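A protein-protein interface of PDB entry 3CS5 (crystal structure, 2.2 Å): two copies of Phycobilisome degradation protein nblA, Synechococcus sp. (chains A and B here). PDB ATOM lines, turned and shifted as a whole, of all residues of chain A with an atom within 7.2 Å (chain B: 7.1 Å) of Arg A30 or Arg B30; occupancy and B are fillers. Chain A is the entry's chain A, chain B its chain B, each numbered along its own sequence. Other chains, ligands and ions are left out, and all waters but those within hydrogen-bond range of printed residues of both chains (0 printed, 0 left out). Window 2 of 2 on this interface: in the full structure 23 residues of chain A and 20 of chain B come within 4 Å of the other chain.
O of Val A25 lies close to OE2 of Glu B34, at 3.0 Å.
Phe B37 touches Val A25. NE of Arg B30 touches NE of Arg A30 (3.5 Å). CD2 of Leu A33 touches O of Arg B30 (3.0 Å). CD2 of Leu A33 touches OE2 of Glu B34, at 3.7 Å. CB of Glu A34 touches CG1 of Val B25 (3.99 Å).
Of the 10 printed residues of chain A, 4 touch a printed residue of chain B. Hydrophobic or aromatic side chains of chain A that line the printed part of chain B: Val A25 and Leu A33. Printed residues of chain B that touch a printed residue of chain A: Val B25, Arg B30, Glu B34 and Phe B37. Along chain B the printed residues that touch a printed residue of chain A span positions 25 to 37.
OE1 of Glu B34 lies close to O of Arg B30 (2.4 Å). The side-chain carboxylate (OE1) of Glu B34 lies close to the backbone NH (N) of Glu B31.
Val A25 touches Glu B34, and with the chains exchanged Glu A34 touches Val B25. Arg A30 touches its own counterpart, Arg B30. Leu A33 touches Arg B30, but with the chains exchanged Arg A30 does not touch Leu B33 (5.5 Å). Leu A33 touches Glu B34, but with the chains exchanged Glu A34 does not touch Leu B33 (4.4 Å). 9 positions are printed for both chains. Of the 6 pairs that touch across the chains among the printed residues, 3 have their exchanged pair printed and touching as well.
Of chain B, only Arg B30 comes within 4 Å of Arg A30. Of chain A, only Arg A30 (3.5 Å) and Leu A33 (3.0 Å) come within 4 Å of Arg B30. Of the printed residues of chain B, Leu A33 touches Arg B30 (3.0 Å) and Glu B34 (3.7 Å). Printed residues of chain B within 4 Å of Glu A34: Val B25 (3.99 Å). Of the printed residues of chain A, Phe B37 touches Val A25 (3.3 Å). Printed residues of chain B within 4 Å of Val A25: Glu B34 (3.0 Å) and Phe B37 (3.3 Å).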
ATOM      1  N   VAL A  25     -14.447 -11.828 -23.781  1.00  0.00           N
ATOM      2  CA  VAL A  25     -15.394 -11.279 -22.840  1.00  0.00           C
ATOM      3  C   VAL A  25     -15.402  -9.762 -22.774  1.00  0.00           C
ATOM      4  O   VAL A  25     -16.312  -9.186 -22.170  1.00  0.00           O
ATOM      5  CB  VAL A  25     -15.069 -11.838 -21.430  1.00  0.00           C
ATOM      6  CG1 VAL A  25     -16.090 -11.378 -20.390  1.00  0.00           C
ATOM      7  CG2 VAL A  25     -14.996 -13.353 -21.507  1.00  0.00           C
ATOM      8  N   ASP A  27     -15.493  -8.038 -25.503  1.00  0.00           N
ATOM      9  CA  ASP A  27     -16.243  -7.770 -26.710  1.00  0.00           C
ATOM     10  C   ASP A  27     -17.678  -8.286 -26.528  1.00  0.00           C
ATOM     11  O   ASP A  27     -18.609  -7.752 -27.135  1.00  0.00           O
ATOM     12  CB  ASP A  27     -15.672  -8.415 -27.975  1.00  0.00           C
ATOM     13  CG  ASP A  27     -14.171  -8.463 -28.094  1.00  0.00           C
ATOM     14  OD1 ASP A  27     -13.558  -7.505 -28.622  1.00  0.00           O
ATOM     15  OD2 ASP A  27     -13.568  -9.475 -27.666  1.00  0.00           O
ATOM     16  N   ILE A  28     -17.822  -9.329 -25.708  1.00  0.00           N
ATOM     17  CA  ILE A  28     -19.143  -9.922 -25.531  1.00  0.00           C
ATOM     18  C   ILE A  28     -20.100  -8.861 -24.965  1.00  0.00           C
ATOM     19  O   ILE A  28     -19.680  -8.079 -24.121  1.00  0.00           O
ATOM     20  CB  ILE A  28     -19.228 -11.142 -24.601  1.00  0.00           C
ATOM     21  CG1 ILE A  28     -18.655 -10.940 -23.179  1.00  0.00           C
ATOM     22  CG2 ILE A  28     -18.582 -12.380 -25.212  1.00  0.00           C
ATOM     23  CD1 ILE A  28     -18.876 -12.234 -22.368  1.00  0.00           C
ATOM     24  N   SER A  29     -21.330  -8.895 -25.459  1.00  0.00           N
ATOM     25  CA  SER A  29     -22.378  -7.958 -25.093  1.00  0.00           C
ATOM     26  C   SER A  29     -22.997  -8.228 -23.723  1.00  0.00           C
ATOM     27  O   SER A  29     -22.706  -9.225 -23.058  1.00  0.00           O
ATOM     28  CB  SER A  29     -23.470  -8.007 -26.171  1.00  0.00           C
ATOM     29  OG  SER A  29     -24.020  -9.307 -26.312  1.00  0.00           O
ATOM     30  N   ARG A  30     -23.864  -7.299 -23.335  1.00  0.00           N
ATOM     31  CA  ARG A  30     -24.593  -7.249 -22.084  1.00  0.00           C
ATOM     32  C   ARG A  30     -25.217  -8.583 -21.686  1.00  0.00           C
ATOM     33  O   ARG A  30     -24.619  -9.272 -20.854  1.00  0.00           O
ATOM     34  CB  ARG A  30     -25.706  -6.190 -22.143  1.00  0.00           C
ATOM     35  CG  ARG A  30     -25.630  -5.169 -21.009  1.00  0.00           C
ATOM     36  CD  ARG A  30     -26.716  -4.118 -21.131  1.00  0.00           C
ATOM     37  NE  ARG A  30     -26.168  -2.755 -21.151  1.00  0.00           N
ATOM     38  CZ  ARG A  30     -26.928  -1.671 -21.208  1.00  0.00           C
ATOM     39  NH1 ARG A  30     -28.248  -1.793 -21.246  1.00  0.00           N
ATOM     40  NH2 ARG A  30     -26.388  -0.465 -21.218  1.00  0.00           N
ATOM     41  N   GLU A  31     -26.381  -8.948 -22.229  1.00  0.00           N
ATOM     42  CA  GLU A  31     -26.999 -10.197 -21.777  1.00  0.00           C
ATOM     43  C   GLU A  31     -26.030 -11.354 -22.071  1.00  0.00           C
ATOM     44  O   GLU A  31     -25.837 -12.220 -21.220  1.00  0.00           O
ATOM     45  CB  GLU A  31     -28.354 -10.524 -22.366  1.00  0.00           C
ATOM     46  CG  GLU A  31     -29.127  -9.477 -23.157  1.00  0.00           C
ATOM     47  CD  GLU A  31     -29.864 -10.130 -24.342  1.00  0.00           C
ATOM     48  OE1 GLU A  31     -29.162 -10.486 -25.329  1.00  0.00           O
ATOM     49  OE2 GLU A  31     -31.116 -10.299 -24.309  1.00  0.00           O
ATOM     50  N   ASP A  32     -25.423 -11.322 -23.249  1.00  0.00           N
ATOM     51  CA  ASP A  32     -24.501 -12.368 -23.681  1.00  0.00           C
ATOM     52  C   ASP A  32     -23.233 -12.423 -22.836  1.00  0.00           C
ATOM     53  O   ASP A  32     -22.418 -13.353 -22.953  1.00  0.00           O
ATOM     54  CB  ASP A  32     -24.146 -12.176 -25.160  1.00  0.00           C
ATOM     55  CG  ASP A  32     -24.663 -13.314 -26.024  1.00  0.00           C
ATOM     56  OD1 ASP A  32     -25.829 -13.734 -25.844  1.00  0.00           O
ATOM     57  OD2 ASP A  32     -23.874 -13.774 -26.882  1.00  0.00           O
ATOM     58  N   LEU A  33     -23.046 -11.445 -21.956  1.00  0.00           N
ATOM     59  CA  LEU A  33     -21.970 -11.537 -20.968  1.00  0.00           C
ATOM     60  C   LEU A  33     -22.583 -11.835 -19.598  1.00  0.00           C
ATOM     61  O   LEU A  33     -21.915 -11.777 -18.568  1.00  0.00           O
ATOM     62  CB  LEU A  33     -21.129 -10.266 -20.987  1.00  0.00           C
ATOM     63  CG  LEU A  33     -20.326  -9.914 -19.722  1.00  0.00           C
ATOM     64  CD1 LEU A  33     -19.206 -10.903 -19.410  1.00  0.00           C
ATOM     65  CD2 LEU A  33     -19.755  -8.490 -19.832  1.00  0.00           C
ATOM     66  N   GLU A  34     -23.873 -12.178 -19.604  1.00  0.00           N
ATOM     67  CA  GLU A  34     -24.618 -12.515 -18.400  1.00  0.00           C
ATOM     68  C   GLU A  34     -24.877 -14.016 -18.254  1.00  0.00           C
ATOM     69  O   GLU A  34     -24.848 -14.546 -17.142  1.00  0.00           O
ATOM     70  CB  GLU A  34     -25.980 -11.813 -18.358  1.00  0.00           C
ATOM     71  CG  GLU A  34     -25.987 -10.328 -18.657  1.00  0.00           C
ATOM     72  CD  GLU A  34     -27.384  -9.734 -18.532  1.00  0.00           C
ATOM     73  OE1 GLU A  34     -28.311 -10.151 -19.252  1.00  0.00           O
ATOM     74  OE2 GLU A  34     -27.573  -8.837 -17.678  1.00  0.00           O
ATOM     75  N   ASP A  35     -25.147 -14.691 -19.363  1.00  0.00           N
ATOM     76  CA  ASP A  35     -25.508 -16.102 -19.372  1.00  0.00           C
ATOM     77  C   ASP A  35     -24.306 -16.993 -19.115  1.00  0.00           C
ATOM     78  O   ASP A  35     -24.411 -18.197 -18.852  1.00  0.00           O
ATOM     79  CB  ASP A  35     -26.172 -16.477 -20.703  1.00  0.00           C
ATOM     80  CG  ASP A  35     -27.681 -16.309 -20.591  1.00  0.00           C
ATOM     81  OD1 ASP A  35     -28.106 -15.454 -19.777  1.00  0.00           O
ATOM     82  OD2 ASP A  35     -28.422 -17.028 -21.296  1.00  0.00           O
ATOM     83  N   VAL B  25     -27.563 -10.903 -10.896  1.00  0.00           N
ATOM     84  CA  VAL B  25     -26.824 -10.544 -12.101  1.00  0.00           C
ATOM     85  C   VAL B  25     -27.608  -9.553 -12.954  1.00  0.00           C
ATOM     86  O   VAL B  25     -27.134  -8.453 -13.239  1.00  0.00           O
ATOM     87  CB  VAL B  25     -26.488 -11.786 -12.948  1.00  0.00           C
ATOM     88  CG1 VAL B  25     -26.593 -11.460 -14.429  1.00  0.00           C
ATOM     89  CG2 VAL B  25     -25.099 -12.302 -12.606  1.00  0.00           C
ATOM     90  N   ILE B  28     -26.628  -6.240 -12.776  1.00  0.00           N
ATOM     91  CA  ILE B  28     -25.211  -5.903 -12.806  1.00  0.00           C
ATOM     92  C   ILE B  28     -24.824  -5.257 -14.132  1.00  0.00           C
ATOM     93  O   ILE B  28     -25.685  -4.808 -14.888  1.00  0.00           O
ATOM     94  CB  ILE B  28     -24.330  -7.146 -12.575  1.00  0.00           C
ATOM     95  CG1 ILE B  28     -24.951  -8.049 -11.507  1.00  0.00           C
ATOM     96  CG2 ILE B  28     -22.921  -6.734 -12.178  1.00  0.00           C
ATOM     97  CD1 ILE B  28     -23.961  -8.982 -10.845  1.00  0.00           C
ATOM     98  N   SER B  29     -23.525  -5.214 -14.407  1.00  0.00           N
ATOM     99  CA  SER B  29     -22.968  -4.227 -15.325  1.00  0.00           C
ATOM    100  C   SER B  29     -21.792  -4.801 -16.107  1.00  0.00           C
ATOM    101  O   SER B  29     -21.047  -5.641 -15.601  1.00  0.00           O
ATOM    102  CB  SER B  29     -22.531  -2.974 -14.562  1.00  0.00           C
ATOM    103  OG  SER B  29     -21.149  -3.022 -14.251  1.00  0.00           O
ATOM    104  N   ARG B  30     -21.632  -4.343 -17.344  1.00  0.00           N
ATOM    105  CA  ARG B  30     -20.663  -4.927 -18.254  1.00  0.00           C
ATOM    106  C   ARG B  30     -19.358  -5.346 -17.588  1.00  0.00           C
ATOM    107  O   ARG B  30     -18.859  -6.441 -17.860  1.00  0.00           O
ATOM    108  CB  ARG B  30     -20.366  -3.925 -19.384  1.00  0.00           C
ATOM    109  CG  ARG B  30     -21.388  -4.001 -20.509  1.00  0.00           C
ATOM    110  CD  ARG B  30     -22.206  -2.726 -20.614  1.00  0.00           C
ATOM    111  NE  ARG B  30     -22.732  -2.551 -21.965  1.00  0.00           N
ATOM    112  CZ  ARG B  30     -22.954  -1.395 -22.574  1.00  0.00           C
ATOM    113  NH1 ARG B  30     -22.714  -0.240 -21.976  1.00  0.00           N
ATOM    114  NH2 ARG B  30     -23.436  -1.417 -23.810  1.00  0.00           N
ATOM    115  N   GLU B  31     -18.807  -4.496 -16.729  1.00  0.00           N
ATOM    116  CA  GLU B  31     -17.527  -4.790 -16.098  1.00  0.00           C
ATOM    117  C   GLU B  31     -17.694  -5.484 -14.749  1.00  0.00           C
ATOM    118  O   GLU B  31     -16.813  -6.243 -14.331  1.00  0.00           O
ATOM    119  CB  GLU B  31     -16.704  -3.510 -15.924  1.00  0.00           C
ATOM    120  CG  GLU B  31     -15.759  -3.212 -17.079  1.00  0.00           C
ATOM    121  CD  GLU B  31     -15.758  -1.739 -17.449  1.00  0.00           C
ATOM    122  OE1 GLU B  31     -16.846  -1.200 -17.742  1.00  0.00           O
ATOM    123  OE2 GLU B  31     -14.680  -1.110 -17.457  1.00  0.00           O
ATOM    124  N   ASP B  32     -18.809  -5.234 -14.054  1.00  0.00           N
ATOM    125  CA  ASP B  32     -18.987  -5.883 -12.751  1.00  0.00           C
ATOM    126  C   ASP B  32     -19.332  -7.359 -12.921  1.00  0.00           C
ATOM    127  O   ASP B  32     -19.142  -8.141 -11.991  1.00  0.00           O
ATOM    128  CB  ASP B  32     -20.051  -5.163 -11.922  1.00  0.00           C
ATOM    129  CG  ASP B  32     -19.393  -4.093 -11.054  1.00  0.00           C
ATOM    130  OD1 ASP B  32     -18.445  -3.440 -11.597  1.00  0.00           O
ATOM    131  OD2 ASP B  32     -19.814  -3.889  -9.811  1.00  0.00           O
ATOM    132  N   LEU B  33     -19.818  -7.736 -14.091  1.00  0.00           N
ATOM    133  CA  LEU B  33     -19.967  -9.155 -14.464  1.00  0.00           C
ATOM    134  C   LEU B  33     -18.715  -9.614 -15.197  1.00  0.00           C
ATOM    135  O   LEU B  33     -18.390 -10.785 -15.098  1.00  0.00           O
ATOM    136  CB  LEU B  33     -21.189  -9.420 -15.364  1.00  0.00           C
ATOM    137  CG  LEU B  33     -22.432  -8.849 -14.616  1.00  0.00           C
ATOM    138  CD1 LEU B  33     -23.626  -8.413 -15.515  1.00  0.00           C
ATOM    139  CD2 LEU B  33     -22.816  -9.808 -13.468  1.00  0.00           C
ATOM    140  N   GLU B  34     -18.090  -8.657 -15.885  1.00  0.00           N
ATOM    141  CA  GLU B  34     -16.807  -8.959 -16.513  1.00  0.00           C
ATOM    142  C   GLU B  34     -15.897  -9.569 -15.436  1.00  0.00           C
ATOM    143  O   GLU B  34     -15.596 -10.747 -15.616  1.00  0.00           O
ATOM    144  CB  GLU B  34     -16.159  -7.742 -17.159  1.00  0.00           C
ATOM    145  CG  GLU B  34     -16.038  -7.833 -18.673  1.00  0.00           C
ATOM    146  CD  GLU B  34     -16.523  -6.579 -19.381  1.00  0.00           C
ATOM    147  OE1 GLU B  34     -16.756  -5.553 -18.700  1.00  0.00           O
ATOM    148  OE2 GLU B  34     -16.675  -6.619 -20.621  1.00  0.00           O
ATOM    149  N   ASP B  35     -15.542  -8.834 -14.396  1.00  0.00           N
ATOM    150  CA  ASP B  35     -14.713  -9.315 -13.305  1.00  0.00           C
ATOM    151  C   ASP B  35     -15.333 -10.519 -12.593  1.00  0.00           C
ATOM    152  O   ASP B  35     -14.619 -11.474 -12.268  1.00  0.00           O
ATOM    153  CB  ASP B  35     -14.461  -8.261 -12.228  1.00  0.00           C
ATOM    154  CG  ASP B  35     -14.059  -6.898 -12.720  1.00  0.00           C
ATOM    155  OD1 ASP B  35     -13.284  -6.813 -13.697  1.00  0.00           O
ATOM    156  OD2 ASP B  35     -14.534  -5.915 -12.098  1.00  0.00           O
ATOM    157  N   PHE B  37     -17.134 -12.535 -13.879  1.00  0.00           N
ATOM    158  CA  PHE B  37     -16.953 -13.567 -14.884  1.00  0.00           C
ATOM    159  C   PHE B  37     -15.487 -13.953 -15.024  1.00  0.00           C
ATOM    160  O   PHE B  37     -15.104 -15.113 -15.031  1.00  0.00           O
ATOM    161  CB  PHE B  37     -17.467 -13.114 -16.268  1.00  0.00           C
ATOM    162  CG  PHE B  37     -17.287 -14.255 -17.270  1.00  0.00           C
ATOM    163  CD1 PHE B  37     -18.154 -15.360 -17.223  1.00  0.00           C
ATOM    164  CD2 PHE B  37     -16.279 -14.218 -18.223  1.00  0.00           C
ATOM    165  CE1 PHE B  37     -18.001 -16.411 -18.109  1.00  0.00           C
ATOM    166  CE2 PHE B  37     -16.125 -15.268 -19.116  1.00  0.00           C
ATOM    167  CZ  PHE B  37     -16.990 -16.364 -19.062  1.00  0.00           C
